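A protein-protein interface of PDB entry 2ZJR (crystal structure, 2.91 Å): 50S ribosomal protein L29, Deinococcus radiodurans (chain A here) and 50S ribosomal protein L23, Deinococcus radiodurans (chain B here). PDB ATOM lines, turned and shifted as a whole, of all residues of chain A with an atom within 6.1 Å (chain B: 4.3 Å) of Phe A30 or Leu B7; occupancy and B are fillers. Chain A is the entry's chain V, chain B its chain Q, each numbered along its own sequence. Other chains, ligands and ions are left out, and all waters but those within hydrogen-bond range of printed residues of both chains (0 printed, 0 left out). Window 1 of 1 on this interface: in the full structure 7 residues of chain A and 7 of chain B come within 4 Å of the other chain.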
ATOM      1  N   LEU A  25      29.888 -16.587   8.555  1.00  0.00           N
ATOM      2  CA  LEU A  25      28.983 -15.712   7.843  1.00  0.00           C
ATOM      3  C   LEU A  25      27.847 -15.238   8.760  1.00  0.00           C
ATOM      4  O   LEU A  25      27.161 -14.257   8.455  1.00  0.00           O
ATOM      5  CB  LEU A  25      28.430 -16.464   6.640  1.00  0.00           C
ATOM      6  CG  LEU A  25      27.758 -15.624   5.568  1.00  0.00           C
ATOM      7  CD1 LEU A  25      28.681 -14.502   5.163  1.00  0.00           C
ATOM      8  CD2 LEU A  25      27.415 -16.493   4.375  1.00  0.00           C
ATOM      9  N   MET A  26      27.635 -15.935   9.875  1.00  0.00           N
ATOM     10  CA  MET A  26      26.597 -15.535  10.813  1.00  0.00           C
ATOM     11  C   MET A  26      27.217 -14.541  11.767  1.00  0.00           C
ATOM     12  O   MET A  26      26.820 -13.381  11.811  1.00  0.00           O
ATOM     13  CB  MET A  26      26.084 -16.720  11.617  1.00  0.00           C
ATOM     14  CG  MET A  26      25.170 -16.315  12.772  1.00  0.00           C
ATOM     15  SD  MET A  26      24.707 -17.686  13.872  1.00  0.00           S
ATOM     16  CE  MET A  26      25.559 -17.221  15.357  1.00  0.00           C
ATOM     17  N   GLU A  27      28.202 -15.000  12.534  1.00  0.00           N
ATOM     18  CA  GLU A  27      28.868 -14.128  13.488  1.00  0.00           C
ATOM     19  C   GLU A  27      29.222 -12.809  12.814  1.00  0.00           C
ATOM     20  O   GLU A  27      29.269 -11.765  13.459  1.00  0.00           O
ATOM     21  CB  GLU A  27      30.123 -14.800  14.040  1.00  0.00           C
ATOM     22  CG  GLU A  27      29.844 -15.975  14.975  1.00  0.00           C
ATOM     23  CD  GLU A  27      28.943 -15.604  16.168  1.00  0.00           C
ATOM     24  OE1 GLU A  27      29.140 -14.520  16.772  1.00  0.00           O
ATOM     25  OE2 GLU A  27      28.042 -16.408  16.517  1.00  0.00           O
ATOM     26  N   LEU A  28      29.475 -12.859  11.511  1.00  0.00           N
ATOM     27  CA  LEU A  28      29.789 -11.645  10.767  1.00  0.00           C
ATOM     28  C   LEU A  28      28.507 -10.828  10.729  1.00  0.00           C
ATOM     29  O   LEU A  28      28.408  -9.742  11.303  1.00  0.00           O
ATOM     30  CB  LEU A  28      30.213 -11.986   9.332  1.00  0.00           C
ATOM     31  CG  LEU A  28      31.670 -12.339   9.036  1.00  0.00           C
ATOM     32  CD1 LEU A  28      32.529 -11.097   9.096  1.00  0.00           C
ATOM     33  CD2 LEU A  28      32.140 -13.377  10.018  1.00  0.00           C
ATOM     34  N   ARG A  29      27.526 -11.387  10.038  1.00  0.00           N
ATOM     35  CA  ARG A  29      26.218 -10.779   9.894  1.00  0.00           C
ATOM     36  C   ARG A  29      25.753 -10.184  11.228  1.00  0.00           C
ATOM     37  O   ARG A  29      25.093  -9.146  11.255  1.00  0.00           O
ATOM     38  CB  ARG A  29      25.247 -11.843   9.387  1.00  0.00           C
ATOM     39  CG  ARG A  29      23.884 -11.349   9.010  1.00  0.00           C
ATOM     40  CD  ARG A  29      23.311 -12.261   7.961  1.00  0.00           C
ATOM     41  NE  ARG A  29      23.677 -13.643   8.219  1.00  0.00           N
ATOM     42  CZ  ARG A  29      23.332 -14.312   9.311  1.00  0.00           C
ATOM     43  NH1 ARG A  29      22.605 -13.723  10.256  1.00  0.00           N
ATOM     44  NH2 ARG A  29      23.714 -15.575   9.464  1.00  0.00           N
ATOM     45  N   PHE A  30      26.095 -10.835  12.335  1.00  0.00           N
ATOM     46  CA  PHE A  30      25.707 -10.294  13.630  1.00  0.00           C
ATOM     47  C   PHE A  30      26.503  -9.011  13.782  1.00  0.00           C
ATOM     48  O   PHE A  30      25.940  -7.920  13.782  1.00  0.00           O
ATOM     49  CB  PHE A  30      26.048 -11.253  14.783  1.00  0.00           C
ATOM     50  CG  PHE A  30      24.925 -12.202  15.155  1.00  0.00           C
ATOM     51  CD1 PHE A  30      24.883 -12.790  16.417  1.00  0.00           C
ATOM     52  CD2 PHE A  30      23.908 -12.501  14.255  1.00  0.00           C
ATOM     53  CE1 PHE A  30      23.841 -13.662  16.770  1.00  0.00           C
ATOM     54  CE2 PHE A  30      22.871 -13.365  14.602  1.00  0.00           C
ATOM     55  CZ  PHE A  30      22.835 -13.944  15.852  1.00  0.00           C
ATOM     56  N   GLN A  31      27.817  -9.151  13.892  1.00  0.00           N
ATOM     57  CA  GLN A  31      28.701  -8.007  14.028  1.00  0.00           C
ATOM     58  C   GLN A  31      28.118  -6.798  13.323  1.00  0.00           C
ATOM     59  O   GLN A  31      27.836  -5.772  13.945  1.00  0.00           O
ATOM     60  CB  GLN A  31      30.065  -8.327  13.434  1.00  0.00           C
ATOM     61  CG  GLN A  31      30.826  -9.333  14.225  1.00  0.00           C
ATOM     62  CD  GLN A  31      32.279  -9.355  13.846  1.00  0.00           C
ATOM     63  OE1 GLN A  31      32.889  -8.300  13.622  1.00  0.00           O
ATOM     64  NE2 GLN A  31      32.861 -10.556  13.783  1.00  0.00           N
ATOM     65  N   ALA A  32      27.935  -6.933  12.015  1.00  0.00           N
ATOM     66  CA  ALA A  32      27.379  -5.852  11.220  1.00  0.00           C
ATOM     67  C   ALA A  32      26.306  -5.140  12.023  1.00  0.00           C
ATOM     68  O   ALA A  32      26.529  -4.034  12.510  1.00  0.00           O
ATOM     69  CB  ALA A  32      26.791  -6.401   9.944  1.00  0.00           C
ATOM     70  N   ALA A  33      25.156  -5.800  12.164  1.00  0.00           N
ATOM     71  CA  ALA A  33      24.006  -5.273  12.902  1.00  0.00           C
ATOM     72  C   ALA A  33      24.390  -4.696  14.258  1.00  0.00           C
ATOM     73  O   ALA A  33      23.777  -3.740  14.732  1.00  0.00           O
ATOM     74  CB  ALA A  33      22.973  -6.359  13.087  1.00  0.00           C
ATOM     75  N   ALA A  34      25.402  -5.284  14.883  1.00  0.00           N
ATOM     76  CA  ALA A  34      25.866  -4.811  16.180  1.00  0.00           C
ATOM     77  C   ALA A  34      26.891  -3.694  15.965  1.00  0.00           C
ATOM     78  O   ALA A  34      27.360  -3.069  16.925  1.00  0.00           O
ATOM     79  CB  ALA A  34      26.493  -5.967  16.975  1.00  0.00           C
ATOM     80  N   GLY A  35      27.229  -3.453  14.701  1.00  0.00           N
ATOM     81  CA  GLY A  35      28.190  -2.420  14.373  1.00  0.00           C
ATOM     82  C   GLY A  35      29.617  -2.788  14.748  1.00  0.00           C
ATOM     83  O   GLY A  35      29.950  -2.898  15.935  1.00  0.00           O
ATOM     84  N   TYR B   4      23.286 -23.032  12.370  1.00  0.00           N
ATOM     85  CA  TYR B   4      23.786 -21.686  12.126  1.00  0.00           C
ATOM     86  C   TYR B   4      23.026 -20.933  11.061  1.00  0.00           C
ATOM     87  O   TYR B   4      23.190 -19.728  10.891  1.00  0.00           O
ATOM     88  CB  TYR B   4      25.270 -21.764  11.799  1.00  0.00           C
ATOM     89  CG  TYR B   4      26.007 -22.433  12.926  1.00  0.00           C
ATOM     90  CD1 TYR B   4      25.647 -22.173  14.252  1.00  0.00           C
ATOM     91  CD2 TYR B   4      27.042 -23.333  12.687  1.00  0.00           C
ATOM     92  CE1 TYR B   4      26.293 -22.789  15.312  1.00  0.00           C
ATOM     93  CE2 TYR B   4      27.706 -23.961  13.751  1.00  0.00           C
ATOM     94  CZ  TYR B   4      27.322 -23.679  15.063  1.00  0.00           C
ATOM     95  OH  TYR B   4      27.972 -24.259  16.134  1.00  0.00           O
ATOM     96  N   ASP B   5      22.178 -21.659  10.356  1.00  0.00           N
ATOM     97  CA  ASP B   5      21.358 -21.074   9.312  1.00  0.00           C
ATOM     98  C   ASP B   5      20.183 -20.379   9.992  1.00  0.00           C
ATOM     99  O   ASP B   5      20.157 -20.263  11.217  1.00  0.00           O
ATOM    100  CB  ASP B   5      20.867 -22.196   8.378  1.00  0.00           C
ATOM    101  CG  ASP B   5      20.577 -23.511   9.124  1.00  0.00           C
ATOM    102  OD1 ASP B   5      20.373 -24.543   8.447  1.00  0.00           O
ATOM    103  OD2 ASP B   5      20.546 -23.513  10.377  1.00  0.00           O
ATOM    104  N   ILE B   6      19.234 -19.898   9.192  1.00  0.00           N
ATOM    105  CA  ILE B   6      18.014 -19.267   9.694  1.00  0.00           C
ATOM    106  C   ILE B   6      18.101 -17.969  10.471  1.00  0.00           C
ATOM    107  O   ILE B   6      17.651 -16.939   9.972  1.00  0.00           O
ATOM    108  CB  ILE B   6      17.181 -20.289  10.496  1.00  0.00           C
ATOM    109  CG1 ILE B   6      16.013 -20.752   9.634  1.00  0.00           C
ATOM    110  CG2 ILE B   6      16.684 -19.705  11.795  1.00  0.00           C
ATOM    111  CD1 ILE B   6      15.086 -21.711  10.331  1.00  0.00           C
ATOM    112  N   LEU B   7      18.644 -17.997  11.685  1.00  0.00           N
ATOM    113  CA  LEU B   7      18.733 -16.768  12.465  1.00  0.00           C
ATOM    114  C   LEU B   7      19.163 -15.722  11.453  1.00  0.00           C
ATOM    115  O   LEU B   7      19.845 -16.050  10.488  1.00  0.00           O
ATOM    116  CB  LEU B   7      19.768 -16.898  13.584  1.00  0.00           C
ATOM    117  CG  LEU B   7      21.232 -16.709  13.188  1.00  0.00           C
ATOM    118  CD1 LEU B   7      21.590 -17.653  12.025  1.00  0.00           C
ATOM    119  CD2 LEU B   7      21.471 -15.249  12.786  1.00  0.00           C
ATOM    120  N   GLN B   8      18.781 -14.469  11.663  1.00  0.00           N
ATOM    121  CA  GLN B   8      19.121 -13.424  10.705  1.00  0.00           C
ATOM    122  C   GLN B   8      20.003 -12.342  11.303  1.00  0.00           C
ATOM    123  O   GLN B   8      20.760 -11.689  10.603  1.00  0.00           O
ATOM    124  CB  GLN B   8      17.836 -12.797  10.162  1.00  0.00           C
ATOM    125  CG  GLN B   8      18.036 -11.974   8.917  1.00  0.00           C
ATOM    126  CD  GLN B   8      18.353 -12.834   7.705  1.00  0.00           C
ATOM    127  OE1 GLN B   8      17.524 -12.978   6.786  1.00  0.00           O
ATOM    128  NE2 GLN B   8      19.554 -13.426   7.697  1.00  0.00           N
ATOM    129  N   ALA B   9      19.893 -12.150  12.606  1.00  0.00           N
ATOM    130  CA  ALA B   9      20.677 -11.140  13.297  1.00  0.00           C
ATOM    131  C   ALA B   9      20.111 -10.963  14.704  1.00  0.00           C
ATOM    132  O   ALA B   9      19.010 -11.434  15.013  1.00  0.00           O
ATOM    133  CB  ALA B   9      20.622  -9.825  12.539  1.00  0.00           C
ATOM    134  N   PRO B  10      20.858 -10.281  15.578  1.00  0.00           N
ATOM    135  CA  PRO B  10      20.405 -10.066  16.945  1.00  0.00           C
ATOM    136  C   PRO B  10      19.564  -8.809  17.080  1.00  0.00           C
ATOM    137  O   PRO B  10      19.828  -7.794  16.436  1.00  0.00           O
ATOM    138  CB  PRO B  10      21.711  -9.951  17.701  1.00  0.00           C
ATOM    139  CG  PRO B  10      22.515  -9.160  16.756  1.00  0.00           C
ATOM    140  CD  PRO B  10      22.243  -9.813  15.417  1.00  0.00           C
ATOM    141  N   TRP B  28      16.456 -11.401  15.505  1.00  0.00           N
ATOM    142  CA  TRP B  28      15.620 -11.464  14.325  1.00  0.00           C
ATOM    143  C   TRP B  28      15.757 -12.738  13.523  1.00  0.00           C
ATOM    144  O   TRP B  28      16.776 -12.937  12.869  1.00  0.00           O
ATOM    145  CB  TRP B  28      15.942 -10.290  13.403  1.00  0.00           C
ATOM    146  CG  TRP B  28      15.691  -9.012  14.033  1.00  0.00           C
ATOM    147  CD1 TRP B  28      16.540  -8.314  14.825  1.00  0.00           C
ATOM    148  CD2 TRP B  28      14.452  -8.309  14.047  1.00  0.00           C
ATOM    149  NE1 TRP B  28      15.904  -7.216  15.350  1.00  0.00           N
ATOM    150  CE2 TRP B  28      14.616  -7.191  14.885  1.00  0.00           C
ATOM    151  CE3 TRP B  28      13.211  -8.520  13.436  1.00  0.00           C
ATOM    152  CZ2 TRP B  28      13.587  -6.286  15.132  1.00  0.00           C
ATOM    153  CZ3 TRP B  28      12.190  -7.620  13.682  1.00  0.00           C
ATOM    154  CH2 TRP B  28      12.384  -6.518  14.522  1.00  0.00           C
ATOM    155  N   PHE B  46      24.314 -21.976  20.031  1.00  0.00           N
ATOM    156  CA  PHE B  46      24.839 -21.380  21.240  1.00  0.00           C
ATOM    157  C   PHE B  46      24.888 -22.415  22.326  1.00  0.00           C
ATOM    158  O   PHE B  46      25.271 -22.137  23.460  1.00  0.00           O
ATOM    159  CB  PHE B  46      23.970 -20.188  21.648  1.00  0.00           C
ATOM    160  CG  PHE B  46      24.016 -19.069  20.657  1.00  0.00           C
ATOM    161  CD1 PHE B  46      23.299 -19.147  19.468  1.00  0.00           C
ATOM    162  CD2 PHE B  46      24.883 -17.991  20.847  1.00  0.00           C
ATOM    163  CE1 PHE B  46      23.450 -18.176  18.473  1.00  0.00           C
ATOM    164  CE2 PHE B  46      25.043 -17.012  19.858  1.00  0.00           C
ATOM    165  CZ  PHE B  46      24.326 -17.107  18.669  1.00  0.00           C
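Of the 11 printed residues of chain A, 3 touch a printed residue of chain B.
Hydrophobic or aromatic side chains of chain A that line the printed part of chain B: Met A26 and Phe A30.
Among the printed residues, 10 pairs touch across the chains.
Phe A30 touches just these residues of chain B: Leu B7, Ala B9, Pro B10 and Phe B46.
Leu B7 touches just these residues of chain A: Met A26, Arg A29 and Phe A30.
Of the printed residues of chain A, Tyr B4 touches Met A26 (3.9 Å).
Of the printed residues of chain A, Ala B9 touches Arg A29 (3.9 Å) and Phe A30 (3.4 Å).
Of the printed residues of chain B, Arg A29 touches Leu B7 (3.2 Å), Gln B8 (2.8 Å) and Ala B9 (3.9 Å).
Printed residues of chain B within 4 Å of Met A26: Tyr B4 (3.9 Å), Leu B7 (3.6 Å) and Phe B46 (3.5 Å).
Glu A27 touches none of the printed residues of chain B.
The nearest printed residue of chain A that does not touch Gln B8 is Phe A30 (4.5 Å).
The backbone carbonyl oxygen of Ala B9 sits at hydrogen-bond distance from the backbone NH of Trp B28 (2.6 Å).
The backbone NH (N) of Gln B8 is in hydrogen-bond range of the backbone carbonyl oxygen (O) of Trp B28, 2.8 Å away.
The guanidinium group of Arg A29 is in hydrogen-bond range of the backbone carbonyl oxygen of Gln B8 (2.8 Å).
Among the printed residues, pairs that only touch across the chains: Phe A30 with Leu B7 (3.0 Å), Arg A29 with Leu B7 (3.2 Å), Phe A30 with Pro B10 (3.4 Å), Phe A30 with Ala B9 (3.4 Å), Met A26 with Phe B46 (3.5 Å), Met A26 with Leu B7 (3.6 Å), Arg A29 with Ala B9 (3.9 Å), Met A26 with Tyr B4 (3.9 Å) and Phe A30 with Phe B46 (3.96 Å).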
